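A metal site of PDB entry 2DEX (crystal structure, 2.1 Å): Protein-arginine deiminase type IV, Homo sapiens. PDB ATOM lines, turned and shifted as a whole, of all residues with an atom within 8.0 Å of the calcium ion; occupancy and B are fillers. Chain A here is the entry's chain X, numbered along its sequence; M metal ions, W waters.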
ATOM      1  N   ASP A 358       1.188 -15.646 -29.014  1.00  0.00           N
ATOM      2  CA  ASP A 358       1.585 -15.841 -27.626  1.00  0.00           C
ATOM      3  C   ASP A 358       0.939 -14.888 -26.620  1.00  0.00           C
ATOM      4  O   ASP A 358       0.685 -15.258 -25.475  1.00  0.00           O
ATOM      5  CB  ASP A 358       3.115 -15.817 -27.531  1.00  0.00           C
ATOM      6  CG  ASP A 358       3.766 -17.040 -28.159  1.00  0.00           C
ATOM      7  OD1 ASP A 358       3.089 -18.108 -28.306  1.00  0.00           O
ATOM      8  OD2 ASP A 358       4.934 -16.934 -28.564  1.00  0.00           O
ATOM      9  N   GLU A 359       0.658 -13.662 -27.036  1.00  0.00           N
ATOM     10  CA  GLU A 359       0.169 -12.648 -26.109  1.00  0.00           C
ATOM     11  C   GLU A 359      -1.333 -12.751 -25.893  1.00  0.00           C
ATOM     12  O   GLU A 359      -1.865 -12.144 -24.960  1.00  0.00           O
ATOM     13  CB  GLU A 359       0.536 -11.253 -26.638  1.00  0.00           C
ATOM     14  CG  GLU A 359       0.347 -10.095 -25.637  1.00  0.00           C
ATOM     15  CD  GLU A 359       1.413 -10.045 -24.547  1.00  0.00           C
ATOM     16  OE1 GLU A 359       1.099  -9.632 -23.409  1.00  0.00           O
ATOM     17  OE2 GLU A 359       2.569 -10.424 -24.796  1.00  0.00           O
ATOM     18  N   MET A 360      -2.056 -13.484 -26.735  1.00  0.00           N
ATOM     19  CA  MET A 360      -3.510 -13.569 -26.567  1.00  0.00           C
ATOM     20  C   MET A 360      -4.183 -14.837 -27.102  1.00  0.00           C
ATOM     21  O   MET A 360      -3.619 -15.578 -27.915  1.00  0.00           O
ATOM     22  CB  MET A 360      -4.160 -12.391 -27.254  1.00  0.00           C
ATOM     23  CG  MET A 360      -4.168 -12.512 -28.748  1.00  0.00           C
ATOM     24  SD  MET A 360      -4.840 -11.063 -29.545  1.00  0.00           S
ATOM     25  CE  MET A 360      -4.875 -11.640 -31.235  1.00  0.00           C
ATOM     26  N   PHE A 376      -8.536 -13.167 -24.172  1.00  0.00           N
ATOM     27  CA  PHE A 376      -7.795 -13.410 -22.945  1.00  0.00           C
ATOM     28  C   PHE A 376      -6.371 -12.951 -23.236  1.00  0.00           C
ATOM     29  O   PHE A 376      -5.694 -13.476 -24.132  1.00  0.00           O
ATOM     30  CB  PHE A 376      -7.847 -14.906 -22.587  1.00  0.00           C
ATOM     31  CG  PHE A 376      -7.224 -15.280 -21.245  1.00  0.00           C
ATOM     32  CD1 PHE A 376      -6.904 -14.335 -20.272  1.00  0.00           C
ATOM     33  CD2 PHE A 376      -6.974 -16.631 -20.972  1.00  0.00           C
ATOM     34  CE1 PHE A 376      -6.346 -14.752 -19.040  1.00  0.00           C
ATOM     35  CE2 PHE A 376      -6.451 -17.052 -19.762  1.00  0.00           C
ATOM     36  CZ  PHE A 376      -6.134 -16.131 -18.787  1.00  0.00           C
ATOM     37  N   ASP A 377      -5.951 -11.938 -22.499  1.00  0.00           N
ATOM     38  CA  ASP A 377      -4.686 -11.262 -22.699  1.00  0.00           C
ATOM     39  C   ASP A 377      -3.671 -11.913 -21.738  1.00  0.00           C
ATOM     40  O   ASP A 377      -3.821 -11.860 -20.521  1.00  0.00           O
ATOM     41  CB  ASP A 377      -4.906  -9.769 -22.425  1.00  0.00           C
ATOM     42  CG  ASP A 377      -3.659  -8.926 -22.571  1.00  0.00           C
ATOM     43  OD1 ASP A 377      -2.590  -9.496 -22.911  1.00  0.00           O
ATOM     44  OD2 ASP A 377      -3.773  -7.679 -22.333  1.00  0.00           O
ATOM     45  N   SER A 378      -2.687 -12.616 -22.298  1.00  0.00           N
ATOM     46  CA  SER A 378      -1.672 -13.302 -21.500  1.00  0.00           C
ATOM     47  C   SER A 378      -0.803 -12.280 -20.757  1.00  0.00           C
ATOM     48  O   SER A 378      -0.477 -11.250 -21.328  1.00  0.00           O
ATOM     49  CB  SER A 378      -0.748 -14.115 -22.410  1.00  0.00           C
ATOM     50  OG  SER A 378       0.508 -14.365 -21.777  1.00  0.00           O
ATOM     51  N   PRO A 379      -0.374 -12.597 -19.514  1.00  0.00           N
ATOM     52  CA  PRO A 379       0.554 -11.741 -18.772  1.00  0.00           C
ATOM     53  C   PRO A 379       1.988 -11.681 -19.314  1.00  0.00           C
ATOM     54  O   PRO A 379       2.821 -10.951 -18.757  1.00  0.00           O
ATOM     55  CB  PRO A 379       0.594 -12.394 -17.385  1.00  0.00           C
ATOM     56  CG  PRO A 379       0.251 -13.798 -17.643  1.00  0.00           C
ATOM     57  CD  PRO A 379      -0.752 -13.779 -18.730  1.00  0.00           C
ATOM     58  N   ARG A 380       2.300 -12.444 -20.361  1.00  0.00           N
ATOM     59  CA  ARG A 380       3.671 -12.448 -20.882  1.00  0.00           C
ATOM     60  C   ARG A 380       4.190 -11.036 -21.164  1.00  0.00           C
ATOM     61  O   ARG A 380       5.346 -10.754 -20.868  1.00  0.00           O
ATOM     62  CB  ARG A 380       3.847 -13.401 -22.061  1.00  0.00           C
ATOM     63  CG  ARG A 380       3.505 -12.886 -23.425  1.00  0.00           C
ATOM     64  CD  ARG A 380       4.431 -13.440 -24.504  1.00  0.00           C
ATOM     65  NE  ARG A 380       4.057 -12.805 -25.755  1.00  0.00           N
ATOM     66  CZ  ARG A 380       4.828 -12.614 -26.819  1.00  0.00           C
ATOM     67  NH1 ARG A 380       6.069 -13.050 -26.911  1.00  0.00           N
ATOM     68  NH2 ARG A 380       4.302 -11.987 -27.853  1.00  0.00           N
ATOM     69  N   ASN A 381       3.335 -10.148 -21.654  1.00  0.00           N
ATOM     70  CA  ASN A 381       3.618  -8.698 -21.730  1.00  0.00           C
ATOM     71  C   ASN A 381       4.957  -8.308 -22.387  1.00  0.00           C
ATOM     72  O   ASN A 381       5.772  -7.554 -21.819  1.00  0.00           O
ATOM     73  CB  ASN A 381       3.533  -8.059 -20.321  1.00  0.00           C
ATOM     74  CG  ASN A 381       2.116  -7.978 -19.801  1.00  0.00           C
ATOM     75  OD1 ASN A 381       1.158  -8.106 -20.571  1.00  0.00           O
ATOM     76  ND2 ASN A 381       1.968  -7.745 -18.493  1.00  0.00           N
ATOM     77  N   ARG A 382       5.152  -8.783 -23.607  1.00  0.00           N
ATOM     78  CA  ARG A 382       6.303  -8.371 -24.388  1.00  0.00           C
ATOM     79  C   ARG A 382       5.876  -7.234 -25.358  1.00  0.00           C
ATOM     80  O   ARG A 382       4.984  -6.447 -25.017  1.00  0.00           O
ATOM     81  CB  ARG A 382       6.947  -9.595 -25.037  1.00  0.00           C
ATOM     82  CG  ARG A 382       7.559 -10.485 -23.947  1.00  0.00           C
ATOM     83  CD  ARG A 382       8.048 -11.791 -24.461  1.00  0.00           C
ATOM     84  NE  ARG A 382       9.225 -11.607 -25.297  1.00  0.00           N
ATOM     85  CZ  ARG A 382       9.773 -12.550 -26.070  1.00  0.00           C
ATOM     86  NH1 ARG A 382       9.244 -13.766 -26.098  1.00  0.00           N
ATOM     87  NH2 ARG A 382      10.855 -12.261 -26.799  1.00  0.00           N
ATOM     88  N   LEU A 384       4.000  -7.026 -27.933  1.00  0.00           N
ATOM     89  CA  LEU A 384       2.567  -7.019 -28.267  1.00  0.00           C
ATOM     90  C   LEU A 384       1.667  -6.659 -27.071  1.00  0.00           C
ATOM     91  O   LEU A 384       0.442  -6.724 -27.184  1.00  0.00           O
ATOM     92  CB  LEU A 384       2.145  -8.388 -28.820  1.00  0.00           C
ATOM     93  CG  LEU A 384       1.935  -8.652 -30.318  1.00  0.00           C
ATOM     94  CD1 LEU A 384       2.236  -7.511 -31.221  1.00  0.00           C
ATOM     95  CD2 LEU A 384       2.711  -9.918 -30.731  1.00  0.00           C
ATOM     96  N   LYS A 385       2.279  -6.280 -25.953  1.00  0.00           N
ATOM     97  CA  LYS A 385       1.570  -5.960 -24.706  1.00  0.00           C
ATOM     98  C   LYS A 385       0.256  -5.179 -24.896  1.00  0.00           C
ATOM     99  O   LYS A 385      -0.773  -5.533 -24.335  1.00  0.00           O
ATOM    100  CB  LYS A 385       2.512  -5.172 -23.766  1.00  0.00           C
ATOM    101  CG  LYS A 385       2.032  -5.128 -22.335  1.00  0.00           C
ATOM    102  CD  LYS A 385       2.938  -4.283 -21.436  1.00  0.00           C
ATOM    103  CE  LYS A 385       2.393  -4.286 -19.988  1.00  0.00           C
ATOM    104  NZ  LYS A 385       2.270  -2.900 -19.405  1.00  0.00           N
ATOM    105  N   GLU A 386       0.301  -4.112 -25.688  1.00  0.00           N
ATOM    106  CA  GLU A 386      -0.835  -3.184 -25.797  1.00  0.00           C
ATOM    107  C   GLU A 386      -1.897  -3.623 -26.812  1.00  0.00           C
ATOM    108  O   GLU A 386      -3.029  -3.140 -26.760  1.00  0.00           O
ATOM    109  CB  GLU A 386      -0.336  -1.777 -26.134  1.00  0.00           C
ATOM    110  CG  GLU A 386       0.588  -1.173 -25.082  1.00  0.00           C
ATOM    111  CD  GLU A 386      -0.044  -1.116 -23.682  1.00  0.00           C
ATOM    112  OE1 GLU A 386       0.732  -1.131 -22.691  1.00  0.00           O
ATOM    113  OE2 GLU A 386      -1.294  -1.074 -23.548  1.00  0.00           O
ATOM    114  N   PHE A 387      -1.535  -4.548 -27.699  1.00  0.00           N
ATOM    115  CA  PHE A 387      -2.386  -4.900 -28.838  1.00  0.00           C
ATOM    116  C   PHE A 387      -3.786  -5.392 -28.433  1.00  0.00           C
ATOM    117  O   PHE A 387      -4.782  -4.916 -28.979  1.00  0.00           O
ATOM    118  CB  PHE A 387      -1.683  -5.918 -29.754  1.00  0.00           C
ATOM    119  CG  PHE A 387      -2.458  -6.239 -31.003  1.00  0.00           C
ATOM    120  CD1 PHE A 387      -2.593  -5.298 -32.008  1.00  0.00           C
ATOM    121  CD2 PHE A 387      -3.039  -7.484 -31.169  1.00  0.00           C
ATOM    122  CE1 PHE A 387      -3.311  -5.583 -33.149  1.00  0.00           C
ATOM    123  CE2 PHE A 387      -3.762  -7.777 -32.313  1.00  0.00           C
ATOM    124  CZ  PHE A 387      -3.896  -6.839 -33.309  1.00  0.00           C
ATOM    125  N   PRO A 388      -3.864  -6.341 -27.487  1.00  0.00           N
ATOM    126  CA  PRO A 388      -5.184  -6.793 -27.037  1.00  0.00           C
ATOM    127  C   PRO A 388      -6.059  -5.694 -26.448  1.00  0.00           C
ATOM    128  O   PRO A 388      -7.261  -5.660 -26.705  1.00  0.00           O
ATOM    129  CB  PRO A 388      -4.842  -7.845 -25.966  1.00  0.00           C
ATOM    130  CG  PRO A 388      -3.472  -8.316 -26.291  1.00  0.00           C
ATOM    131  CD  PRO A 388      -2.775  -7.080 -26.820  1.00  0.00           C
ATOM    132  N   ILE A 389      -5.432  -4.783 -25.704  1.00  0.00           N
ATOM    133  CA  ILE A 389      -6.151  -3.738 -24.981  1.00  0.00           C
ATOM    134  C   ILE A 389      -6.541  -2.609 -25.935  1.00  0.00           C
ATOM    135  O   ILE A 389      -7.686  -2.134 -25.907  1.00  0.00           O
ATOM    136  CB  ILE A 389      -5.298  -3.148 -23.803  1.00  0.00           C
ATOM    137  CG1 ILE A 389      -4.483  -4.231 -23.086  1.00  0.00           C
ATOM    138  CG2 ILE A 389      -6.203  -2.485 -22.780  1.00  0.00           C
ATOM    139  CD1 ILE A 389      -3.554  -3.671 -21.998  1.00  0.00           C
ATOM    140  N   TYR A 399     -12.708  -8.210 -23.092  1.00  0.00           N
ATOM    141  CA  TYR A 399     -11.360  -8.346 -22.580  1.00  0.00           C
ATOM    142  C   TYR A 399     -11.349  -9.092 -21.238  1.00  0.00           C
ATOM    143  O   TYR A 399     -12.251  -8.890 -20.424  1.00  0.00           O
ATOM    144  CB  TYR A 399     -10.772  -6.955 -22.390  1.00  0.00           C
ATOM    145  CG  TYR A 399      -9.327  -6.961 -21.939  1.00  0.00           C
ATOM    146  CD1 TYR A 399      -8.295  -7.007 -22.848  1.00  0.00           C
ATOM    147  CD2 TYR A 399      -9.011  -6.934 -20.580  1.00  0.00           C
ATOM    148  CE1 TYR A 399      -6.982  -7.037 -22.443  1.00  0.00           C
ATOM    149  CE2 TYR A 399      -7.691  -6.959 -20.163  1.00  0.00           C
ATOM    150  CZ  TYR A 399      -6.687  -7.016 -21.095  1.00  0.00           C
ATOM    151  OH  TYR A 399      -5.377  -7.023 -20.671  1.00  0.00           O
ATOM    152  N   VAL A 400     -10.339  -9.949 -21.042  1.00  0.00           N
ATOM    153  CA  VAL A 400      -9.979 -10.537 -19.740  1.00  0.00           C
ATOM    154  C   VAL A 400      -8.463 -10.710 -19.656  1.00  0.00           C
ATOM    155  O   VAL A 400      -7.789 -11.054 -20.643  1.00  0.00           O
ATOM    156  CB  VAL A 400     -10.490 -12.000 -19.520  1.00  0.00           C
ATOM    157  CG1 VAL A 400     -10.882 -12.239 -18.019  1.00  0.00           C
ATOM    158  CG2 VAL A 400     -11.597 -12.377 -20.455  1.00  0.00           C
ATOM    159  N   THR A 401      -7.921 -10.556 -18.461  1.00  0.00           N
ATOM    160  CA  THR A 401      -6.525 -10.902 -18.214  1.00  0.00           C
ATOM    161  C   THR A 401      -6.390 -11.525 -16.829  1.00  0.00           C
ATOM    162  O   THR A 401      -7.283 -11.385 -16.008  1.00  0.00           O
ATOM    163  CB  THR A 401      -5.606  -9.707 -18.382  1.00  0.00           C
ATOM    164  OG1 THR A 401      -4.257 -10.150 -18.513  1.00  0.00           O
ATOM    165  CG2 THR A 401      -5.748  -8.739 -17.209  1.00  0.00           C
ATOM    166  N   ARG A 402      -5.296 -12.262 -16.634  1.00  0.00           N
ATOM    167  CA  ARG A 402      -4.997 -12.926 -15.358  1.00  0.00           C
ATOM    168  C   ARG A 402      -3.487 -13.012 -15.166  1.00  0.00           C
ATOM    169  O   ARG A 402      -2.713 -12.901 -16.121  1.00  0.00           O
ATOM    170  CB  ARG A 402      -5.555 -14.346 -15.303  1.00  0.00           C
ATOM    171  CG  ARG A 402      -7.067 -14.473 -15.148  1.00  0.00           C
ATOM    172  CD  ARG A 402      -7.486 -13.887 -13.843  1.00  0.00           C
ATOM    173  NE  ARG A 402      -8.865 -14.170 -13.476  1.00  0.00           N
ATOM    174  CZ  ARG A 402      -9.903 -13.411 -13.783  1.00  0.00           C
ATOM    175  NH1 ARG A 402      -9.751 -12.346 -14.548  1.00  0.00           N
ATOM    176  NH2 ARG A 402     -11.114 -13.723 -13.337  1.00  0.00           N
ATOM    177  N   PRO A 404       0.198 -12.213 -12.632  1.00  0.00           N
ATOM    178  CA  PRO A 404       0.930 -10.991 -12.332  1.00  0.00           C
ATOM    179  C   PRO A 404       1.415 -10.322 -13.607  1.00  0.00           C
ATOM    180  O   PRO A 404       1.866 -11.011 -14.535  1.00  0.00           O
ATOM    181  CB  PRO A 404       2.118 -11.486 -11.489  1.00  0.00           C
ATOM    182  CG  PRO A 404       2.287 -12.915 -11.865  1.00  0.00           C
ATOM    183  CD  PRO A 404       0.913 -13.422 -12.196  1.00  0.00           C
ATOM    184  N   GLN A 405       1.350  -8.993 -13.639  1.00  0.00           N
ATOM    185  CA  GLN A 405       1.576  -8.260 -14.878  1.00  0.00           C
ATOM    186  C   GLN A 405       2.952  -7.571 -14.992  1.00  0.00           C
ATOM    187  O   GLN A 405       3.302  -7.125 -16.079  1.00  0.00           O
ATOM    188  CB  GLN A 405       0.439  -7.258 -15.119  1.00  0.00           C
ATOM    189  CG  GLN A 405      -0.980  -7.885 -15.119  1.00  0.00           C
ATOM    190  CD  GLN A 405      -1.294  -8.693 -16.382  1.00  0.00           C
ATOM    191  OE1 GLN A 405      -0.793  -8.404 -17.482  1.00  0.00           O
ATOM    192  NE2 GLN A 405      -2.162  -9.695 -16.238  1.00  0.00           N
ATOM    193  N   PHE A 415       0.639 -17.881 -24.918  1.00  0.00           N
ATOM    194  CA  PHE A 415      -0.567 -18.619 -25.281  1.00  0.00           C
ATOM    195  C   PHE A 415      -0.444 -19.542 -26.500  1.00  0.00           C
ATOM    196  O   PHE A 415      -1.435 -20.129 -26.952  1.00  0.00           O
ATOM    197  CB  PHE A 415      -1.771 -17.669 -25.335  1.00  0.00           C
ATOM    198  CG  PHE A 415      -2.290 -17.238 -23.967  1.00  0.00           C
ATOM    199  CD1 PHE A 415      -3.244 -16.254 -23.859  1.00  0.00           C
ATOM    200  CD2 PHE A 415      -1.807 -17.832 -22.780  1.00  0.00           C
ATOM    201  CE1 PHE A 415      -3.752 -15.841 -22.616  1.00  0.00           C
ATOM    202  CE2 PHE A 415      -2.302 -17.458 -21.531  1.00  0.00           C
ATOM    203  CZ  PHE A 415      -3.267 -16.441 -21.452  1.00  0.00           C
HETATM  204 CA    CA M   1      -0.431  -9.047 -21.789  1.00  0.00          CA
HETATM  205  O   HOH W   1      -1.865  -8.715 -19.745  1.00  0.00           O
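Water W1 lies within hydrogen-bond range of OE1 of Gln 405 (2.5 Å), OG1 of Thr 401 (3.0 Å) and OD2 of Asp 377 (3.4 Å).
The backbone carbonyl oxygen of Asp 377 is in hydrogen-bond range of the side-chain hydroxyl of Thr 401 (2.7 Å).
The side-chain carboxylate of Asp 377 sits at hydrogen-bond distance from the side-chain hydroxyl of Tyr 399 (2.4 Å).
The side-chain carboxylate (OE2) of Glu 359 is in salt-bridge range of the guanidinium group (NE) of Arg 380 (3.0 Å).
OG of Ser 378 is in hydrogen-bond range of N of Arg 380, 3.0 Å away.
The side-chain amide nitrogen of Asn 381 sits at hydrogen-bond distance from the backbone carbonyl oxygen of Gln 405.
OE2 of Glu 359 is in hydrogen-bond range of N of Arg 382, 3.3 Å away.
ND2 of Asn 381 sits close to O of Pro 379 (3.3 Å).
The backbone NH (N) of Asp 377 sits at hydrogen-bond distance from the backbone carbonyl oxygen (O) of Val 400 (2.8 Å).
The calcium ion is bound by the side-chain amide oxygen of Asn 381 (2.2 Å), the backbone carbonyl oxygen of Ser 378 (2.3 Å), the side-chain carboxylate of Glu 359 (2.3 Å), the side-chain carboxylate of Asp 377 (2.5 Å) and water W1 (2.5 Å).
Of the 23 residues printed, 4 come within 4 Å of the calcium ion.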
